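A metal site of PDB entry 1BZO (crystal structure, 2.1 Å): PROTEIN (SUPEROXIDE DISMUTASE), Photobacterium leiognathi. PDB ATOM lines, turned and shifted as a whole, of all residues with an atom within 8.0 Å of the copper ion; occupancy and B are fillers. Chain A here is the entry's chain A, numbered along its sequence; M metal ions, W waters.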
ATOM      1  N   GLY A  43      -0.918  16.583  -5.533  1.00  0.00           N
ATOM      2  CA  GLY A  43      -2.278  16.779  -5.942  1.00  0.00           C
ATOM      3  C   GLY A  43      -3.080  17.216  -4.737  1.00  0.00           C
ATOM      4  O   GLY A  43      -2.918  16.682  -3.642  1.00  0.00           O
ATOM      5  N   PHE A  44      -3.955  18.188  -4.923  1.00  0.00           N
ATOM      6  CA  PHE A  44      -4.725  18.733  -3.832  1.00  0.00           C
ATOM      7  C   PHE A  44      -6.174  18.903  -4.317  1.00  0.00           C
ATOM      8  O   PHE A  44      -6.354  19.602  -5.300  1.00  0.00           O
ATOM      9  CB  PHE A  44      -4.142  20.140  -3.661  1.00  0.00           C
ATOM     10  CG  PHE A  44      -4.599  20.991  -2.477  1.00  0.00           C
ATOM     11  CD1 PHE A  44      -4.868  20.430  -1.229  1.00  0.00           C
ATOM     12  CD2 PHE A  44      -4.625  22.390  -2.611  1.00  0.00           C
ATOM     13  CE1 PHE A  44      -5.241  21.226  -0.129  1.00  0.00           C
ATOM     14  CE2 PHE A  44      -4.885  23.201  -1.507  1.00  0.00           C
ATOM     15  CZ  PHE A  44      -5.186  22.618  -0.271  1.00  0.00           C
ATOM     16  N   HIS A  45      -7.215  18.291  -3.661  1.00  0.00           N
ATOM     17  CA  HIS A  45      -8.632  18.356  -4.132  1.00  0.00           C
ATOM     18  C   HIS A  45      -9.614  18.255  -2.993  1.00  0.00           C
ATOM     19  O   HIS A  45      -9.270  17.760  -1.882  1.00  0.00           O
ATOM     20  CB  HIS A  45      -8.942  17.145  -5.036  1.00  0.00           C
ATOM     21  CG  HIS A  45      -7.825  16.682  -5.878  1.00  0.00           C
ATOM     22  ND1 HIS A  45      -7.222  15.454  -5.699  1.00  0.00           N
ATOM     23  CD2 HIS A  45      -7.151  17.321  -6.886  1.00  0.00           C
ATOM     24  CE1 HIS A  45      -6.258  15.336  -6.608  1.00  0.00           C
ATOM     25  NE2 HIS A  45      -6.187  16.461  -7.353  1.00  0.00           N
ATOM     26  N   ILE A  46     -10.828  18.697  -3.293  1.00  0.00           N
ATOM     27  CA  ILE A  46     -11.968  18.588  -2.381  1.00  0.00           C
ATOM     28  C   ILE A  46     -12.584  17.266  -2.786  1.00  0.00           C
ATOM     29  O   ILE A  46     -12.722  17.032  -4.008  1.00  0.00           O
ATOM     30  CB  ILE A  46     -13.055  19.671  -2.551  1.00  0.00           C
ATOM     31  CG1 ILE A  46     -12.443  21.084  -2.526  1.00  0.00           C
ATOM     32  CG2 ILE A  46     -14.172  19.532  -1.472  1.00  0.00           C
ATOM     33  CD1 ILE A  46     -11.873  21.557  -1.181  1.00  0.00           C
ATOM     34  N   HIS A  47     -12.779  16.384  -1.799  1.00  0.00           N
ATOM     35  CA  HIS A  47     -13.399  15.066  -1.999  1.00  0.00           C
ATOM     36  C   HIS A  47     -14.844  15.138  -1.519  1.00  0.00           C
ATOM     37  O   HIS A  47     -15.237  16.079  -0.758  1.00  0.00           O
ATOM     38  CB  HIS A  47     -12.613  13.860  -1.379  1.00  0.00           C
ATOM     39  CG  HIS A  47     -11.464  13.452  -2.224  1.00  0.00           C
ATOM     40  ND1 HIS A  47     -11.342  12.169  -2.722  1.00  0.00           N
ATOM     41  CD2 HIS A  47     -10.363  14.174  -2.600  1.00  0.00           C
ATOM     42  CE1 HIS A  47     -10.200  12.126  -3.423  1.00  0.00           C
ATOM     43  NE2 HIS A  47      -9.615  13.328  -3.391  1.00  0.00           N
ATOM     44  N   GLY A  68     -14.431   9.194  -0.342  1.00  0.00           N
ATOM     45  CA  GLY A  68     -14.981   9.026  -1.693  1.00  0.00           C
ATOM     46  C   GLY A  68     -14.066   9.669  -2.758  1.00  0.00           C
ATOM     47  O   GLY A  68     -12.841   9.881  -2.532  1.00  0.00           O
ATOM     48  N   GLY A  69     -14.680  10.010  -3.931  1.00  0.00           N
ATOM     49  CA  GLY A  69     -13.966  10.563  -5.098  1.00  0.00           C
ATOM     50  C   GLY A  69     -13.857  12.074  -5.009  1.00  0.00           C
ATOM     51  O   GLY A  69     -14.251  12.626  -3.997  1.00  0.00           O
ATOM     52  N   HIS A  70     -13.437  12.753  -6.080  1.00  0.00           N
ATOM     53  CA  HIS A  70     -13.346  14.261  -6.109  1.00  0.00           C
ATOM     54  C   HIS A  70     -14.735  14.951  -6.005  1.00  0.00           C
ATOM     55  O   HIS A  70     -15.759  14.489  -6.513  1.00  0.00           O
ATOM     56  CB  HIS A  70     -12.639  14.709  -7.437  1.00  0.00           C
ATOM     57  CG  HIS A  70     -11.214  14.233  -7.528  1.00  0.00           C
ATOM     58  ND1 HIS A  70     -10.361  14.632  -8.570  1.00  0.00           N
ATOM     59  CD2 HIS A  70     -10.476  13.469  -6.624  1.00  0.00           C
ATOM     60  CE1 HIS A  70      -9.142  14.119  -8.305  1.00  0.00           C
ATOM     61  NE2 HIS A  70      -9.178  13.389  -7.144  1.00  0.00           N
ATOM     62  N   TYR A  71     -14.832  16.101  -5.393  1.00  0.00           N
ATOM     63  CA  TYR A  71     -16.125  16.796  -5.334  1.00  0.00           C
ATOM     64  C   TYR A  71     -16.546  17.060  -6.791  1.00  0.00           C
ATOM     65  O   TYR A  71     -15.779  17.551  -7.612  1.00  0.00           O
ATOM     66  CB  TYR A  71     -15.985  18.103  -4.474  1.00  0.00           C
ATOM     67  CG  TYR A  71     -17.208  19.029  -4.366  1.00  0.00           C
ATOM     68  CD1 TYR A  71     -18.484  18.558  -4.037  1.00  0.00           C
ATOM     69  CD2 TYR A  71     -17.061  20.397  -4.596  1.00  0.00           C
ATOM     70  CE1 TYR A  71     -19.579  19.421  -3.879  1.00  0.00           C
ATOM     71  CE2 TYR A  71     -18.133  21.287  -4.515  1.00  0.00           C
ATOM     72  CZ  TYR A  71     -19.397  20.782  -4.127  1.00  0.00           C
ATOM     73  OH  TYR A  71     -20.450  21.650  -3.982  1.00  0.00           O
ATOM     74  N   HIS A  79     -11.621  14.667 -14.716  1.00  0.00           N
ATOM     75  CA  HIS A  79     -10.646  15.391 -13.898  1.00  0.00           C
ATOM     76  C   HIS A  79      -9.977  16.508 -14.705  1.00  0.00           C
ATOM     77  O   HIS A  79      -9.536  16.322 -15.837  1.00  0.00           O
ATOM     78  CB  HIS A  79      -9.609  14.467 -13.273  1.00  0.00           C
ATOM     79  CG  HIS A  79      -8.658  15.254 -12.407  1.00  0.00           C
ATOM     80  ND1 HIS A  79      -9.058  15.773 -11.216  1.00  0.00           N
ATOM     81  CD2 HIS A  79      -7.322  15.547 -12.580  1.00  0.00           C
ATOM     82  CE1 HIS A  79      -8.001  16.343 -10.647  1.00  0.00           C
ATOM     83  NE2 HIS A  79      -6.916  16.214 -11.453  1.00  0.00           N
ATOM     84  N   HIS A  88     -14.322  17.870 -12.355  1.00  0.00           N
ATOM     85  CA  HIS A  88     -14.697  18.059 -10.973  1.00  0.00           C
ATOM     86  C   HIS A  88     -14.603  19.469 -10.443  1.00  0.00           C
ATOM     87  O   HIS A  88     -13.598  20.166 -10.589  1.00  0.00           O
ATOM     88  CB  HIS A  88     -13.831  17.223 -10.036  1.00  0.00           C
ATOM     89  CG  HIS A  88     -13.676  15.863 -10.599  1.00  0.00           C
ATOM     90  ND1 HIS A  88     -12.439  15.235 -10.709  1.00  0.00           N
ATOM     91  CD2 HIS A  88     -14.596  15.024 -11.101  1.00  0.00           C
ATOM     92  CE1 HIS A  88     -12.636  14.047 -11.217  1.00  0.00           C
ATOM     93  NE2 HIS A  88     -13.939  13.907 -11.486  1.00  0.00           N
ATOM     94  N   GLY A  90     -14.220  19.932  -7.416  1.00  0.00           N
ATOM     95  CA  GLY A  90     -13.169  20.108  -6.353  1.00  0.00           C
ATOM     96  C   GLY A  90     -11.697  19.998  -6.794  1.00  0.00           C
ATOM     97  O   GLY A  90     -10.805  19.753  -5.991  1.00  0.00           O
ATOM     98  N   ASP A  91     -11.426  20.206  -8.048  1.00  0.00           N
ATOM     99  CA  ASP A  91     -10.055  20.198  -8.557  1.00  0.00           C
ATOM    100  C   ASP A  91      -9.386  21.565  -8.259  1.00  0.00           C
ATOM    101  O   ASP A  91      -9.714  22.624  -8.833  1.00  0.00           O
ATOM    102  CB  ASP A  91     -10.130  20.033 -10.105  1.00  0.00           C
ATOM    103  CG  ASP A  91     -10.541  18.641 -10.413  1.00  0.00           C
ATOM    104  OD1 ASP A  91     -10.472  17.815  -9.505  1.00  0.00           O
ATOM    105  OD2 ASP A  91     -10.923  18.410 -11.680  1.00  0.00           O
ATOM    106  N   ALA A 121     -14.373  17.027   2.468  1.00  0.00           N
ATOM    107  CA  ALA A 121     -13.049  16.703   2.967  1.00  0.00           C
ATOM    108  C   ALA A 121     -11.946  17.265   2.093  1.00  0.00           C
ATOM    109  O   ALA A 121     -12.078  17.166   0.866  1.00  0.00           O
ATOM    110  CB  ALA A 121     -12.813  15.201   3.017  1.00  0.00           C
ATOM    111  N   ILE A 122     -10.871  17.793   2.681  1.00  0.00           N
ATOM    112  CA  ILE A 122      -9.739  18.234   1.839  1.00  0.00           C
ATOM    113  C   ILE A 122      -8.698  17.118   1.838  1.00  0.00           C
ATOM    114  O   ILE A 122      -8.284  16.695   2.927  1.00  0.00           O
ATOM    115  CB  ILE A 122      -9.062  19.526   2.356  1.00  0.00           C
ATOM    116  CG1 ILE A 122     -10.125  20.575   2.432  1.00  0.00           C
ATOM    117  CG2 ILE A 122      -7.892  20.063   1.439  1.00  0.00           C
ATOM    118  CD1 ILE A 122     -10.118  21.386   1.147  1.00  0.00           C
ATOM    119  N   MET A 123      -8.203  16.734   0.663  1.00  0.00           N
ATOM    120  CA  MET A 123      -7.158  15.691   0.486  1.00  0.00           C
ATOM    121  C   MET A 123      -5.826  16.166  -0.096  1.00  0.00           C
ATOM    122  O   MET A 123      -5.821  16.870  -1.103  1.00  0.00           O
ATOM    123  CB  MET A 123      -7.640  14.666  -0.578  1.00  0.00           C
ATOM    124  CG  MET A 123      -7.041  13.254  -0.327  1.00  0.00           C
ATOM    125  SD  MET A 123      -7.578  12.559   1.310  1.00  0.00           S
ATOM    126  CE  MET A 123      -9.368  12.196   0.986  1.00  0.00           C
ATOM    127  N   ILE A 124      -4.704  15.645   0.436  1.00  0.00           N
ATOM    128  CA  ILE A 124      -3.363  15.909  -0.140  1.00  0.00           C
ATOM    129  C   ILE A 124      -2.868  14.530  -0.605  1.00  0.00           C
ATOM    130  O   ILE A 124      -2.974  13.560   0.115  1.00  0.00           O
ATOM    131  CB  ILE A 124      -2.341  16.609   0.809  1.00  0.00           C
ATOM    132  CG1 ILE A 124      -2.828  18.032   1.156  1.00  0.00           C
ATOM    133  CG2 ILE A 124      -0.871  16.658   0.264  1.00  0.00           C
ATOM    134  CD1 ILE A 124      -2.153  18.731   2.356  1.00  0.00           C
ATOM    135  N   HIS A 125      -2.433  14.422  -1.860  1.00  0.00           N
ATOM    136  CA  HIS A 125      -1.937  13.133  -2.409  1.00  0.00           C
ATOM    137  C   HIS A 125      -0.437  13.024  -2.401  1.00  0.00           C
ATOM    138  O   HIS A 125       0.239  14.018  -2.264  1.00  0.00           O
ATOM    139  CB  HIS A 125      -2.405  12.971  -3.883  1.00  0.00           C
ATOM    140  CG  HIS A 125      -3.863  12.757  -3.889  1.00  0.00           C
ATOM    141  ND1 HIS A 125      -4.416  11.503  -4.073  1.00  0.00           N
ATOM    142  CD2 HIS A 125      -4.862  13.657  -3.703  1.00  0.00           C
ATOM    143  CE1 HIS A 125      -5.749  11.656  -3.992  1.00  0.00           C
ATOM    144  NE2 HIS A 125      -6.035  12.945  -3.759  1.00  0.00           N
ATOM    145  N   ASP A 129      -0.169  16.578  -9.825  1.00  0.00           N
ATOM    146  CA  ASP A 129      -1.479  16.762 -10.415  1.00  0.00           C
ATOM    147  C   ASP A 129      -1.297  17.280 -11.831  1.00  0.00           C
ATOM    148  O   ASP A 129      -0.999  18.464 -11.956  1.00  0.00           O
ATOM    149  CB  ASP A 129      -2.432  17.690  -9.606  1.00  0.00           C
ATOM    150  CG  ASP A 129      -3.847  17.629 -10.185  1.00  0.00           C
ATOM    151  OD1 ASP A 129      -4.076  17.255 -11.311  1.00  0.00           O
ATOM    152  OD2 ASP A 129      -4.834  17.917  -9.363  1.00  0.00           O
ATOM    153  N   LEU A 138      -6.911  10.566 -12.591  1.00  0.00           N
ATOM    154  CA  LEU A 138      -6.986  11.612 -11.603  1.00  0.00           C
ATOM    155  C   LEU A 138      -5.736  12.474 -11.471  1.00  0.00           C
ATOM    156  O   LEU A 138      -5.394  12.941 -10.398  1.00  0.00           O
ATOM    157  CB  LEU A 138      -7.463  11.019 -10.253  1.00  0.00           C
ATOM    158  CG  LEU A 138      -8.912  10.502 -10.320  1.00  0.00           C
ATOM    159  CD1 LEU A 138      -9.109   9.362  -9.338  1.00  0.00           C
ATOM    160  CD2 LEU A 138      -9.837  11.592  -9.770  1.00  0.00           C
ATOM    161  N   GLY A 141      -2.175  11.730  -8.960  1.00  0.00           N
ATOM    162  CA  GLY A 141      -1.934  11.952  -7.524  1.00  0.00           C
ATOM    163  C   GLY A 141      -1.598  10.654  -6.722  1.00  0.00           C
ATOM    164  O   GLY A 141      -0.878  10.674  -5.677  1.00  0.00           O
ATOM    165  N   GLY A 142      -2.219   9.542  -7.156  1.00  0.00           N
ATOM    166  CA  GLY A 142      -2.047   8.266  -6.496  1.00  0.00           C
ATOM    167  C   GLY A 142      -2.606   8.245  -5.084  1.00  0.00           C
ATOM    168  O   GLY A 142      -3.695   8.722  -4.830  1.00  0.00           O
ATOM    169  N   ALA A 143      -1.812   7.685  -4.130  1.00  0.00           N
ATOM    170  CA  ALA A 143      -2.215   7.532  -2.747  1.00  0.00           C
ATOM    171  C   ALA A 143      -2.595   8.865  -2.097  1.00  0.00           C
ATOM    172  O   ALA A 143      -2.095   9.906  -2.497  1.00  0.00           O
ATOM    173  CB  ALA A 143      -1.049   6.893  -1.954  1.00  0.00           C
ATOM    174  N   ARG A 144      -3.400   8.794  -1.026  1.00  0.00           N
ATOM    175  CA  ARG A 144      -3.771   9.975  -0.241  1.00  0.00           C
ATOM    176  C   ARG A 144      -2.825  10.021   0.947  1.00  0.00           C
ATOM    177  O   ARG A 144      -2.570   9.009   1.631  1.00  0.00           O
ATOM    178  CB  ARG A 144      -5.228   9.834   0.235  1.00  0.00           C
ATOM    179  CG  ARG A 144      -6.223   9.592  -0.918  1.00  0.00           C
ATOM    180  CD  ARG A 144      -7.608   8.995  -0.489  1.00  0.00           C
ATOM    181  NE  ARG A 144      -8.517   8.794  -1.651  1.00  0.00           N
ATOM    182  CZ  ARG A 144      -9.843   9.061  -1.763  1.00  0.00           C
ATOM    183  NH1 ARG A 144     -10.608   9.565  -0.785  1.00  0.00           N
ATOM    184  NH2 ARG A 144     -10.381   8.843  -2.949  1.00  0.00           N
ATOM    185  N   ALA A 146      -2.521  13.042   3.241  1.00  0.00           N
ATOM    186  CA  ALA A 146      -3.040  13.870   4.338  1.00  0.00           C
ATOM    187  C   ALA A 146      -4.504  14.271   4.143  1.00  0.00           C
ATOM    188  O   ALA A 146      -4.949  14.557   3.017  1.00  0.00           O
ATOM    189  CB  ALA A 146      -2.116  14.975   4.809  1.00  0.00           C
HETATM  190 CU    CU M   1      -7.914  13.998  -4.302  1.00  0.00          CU
HETATM  191 ZN    ZN M   2     -10.624  15.813 -10.098  1.00  0.00          ZN
HETATM  192  O   HOH W   1      -8.339  10.904  -5.819  1.00  0.00           O
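The copper ion is bound by a ring nitrogen (NE2) of His 47 (2.0 Å), a ring nitrogen (ND1) of His 45 (2.1 Å) and a ring nitrogen (NE2) of His 125 (2.2 Å).
O of His 45 sits at hydrogen-bond distance from N of Met 123 (2.9 Å). A ring nitrogen (NE2) of His 45 lies within hydrogen-bond range of the side-chain carboxylate (OD2) of Asp 129 (2.8 Å). The backbone NH (N) of His 125 sits at hydrogen-bond distance from the backbone carbonyl oxygen (O) of Gly 43 (2.9 Å). ND1 of His 47 is in hydrogen-bond range of O of Gly 68 (2.7 Å). The guanidinium group (NH1) of Arg 144 lies within hydrogen-bond range of a ring nitrogen (ND1) of His 47. A ring nitrogen (ND1) of His 47 is in hydrogen-bond range of the backbone carbonyl oxygen (O) of Gly 69. ND1 of His 125 is in hydrogen-bond range of O of Gly 142, at 3.0 Å. The backbone NH (N) of His 47 sits at hydrogen-bond distance from the backbone carbonyl oxygen (O) of Ala 121 (2.9 Å).
His 70 touches the copper ion (NE2 to CU, 3.2 Å). CB of Met 123 touches the copper ion (3.8 Å). Within 4 Å of the copper ion: His 45, His 47, His 70, Met 123 and His 125. The nearest printed residue that does not touch the copper ion is Phe 44 (5.2 Å).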
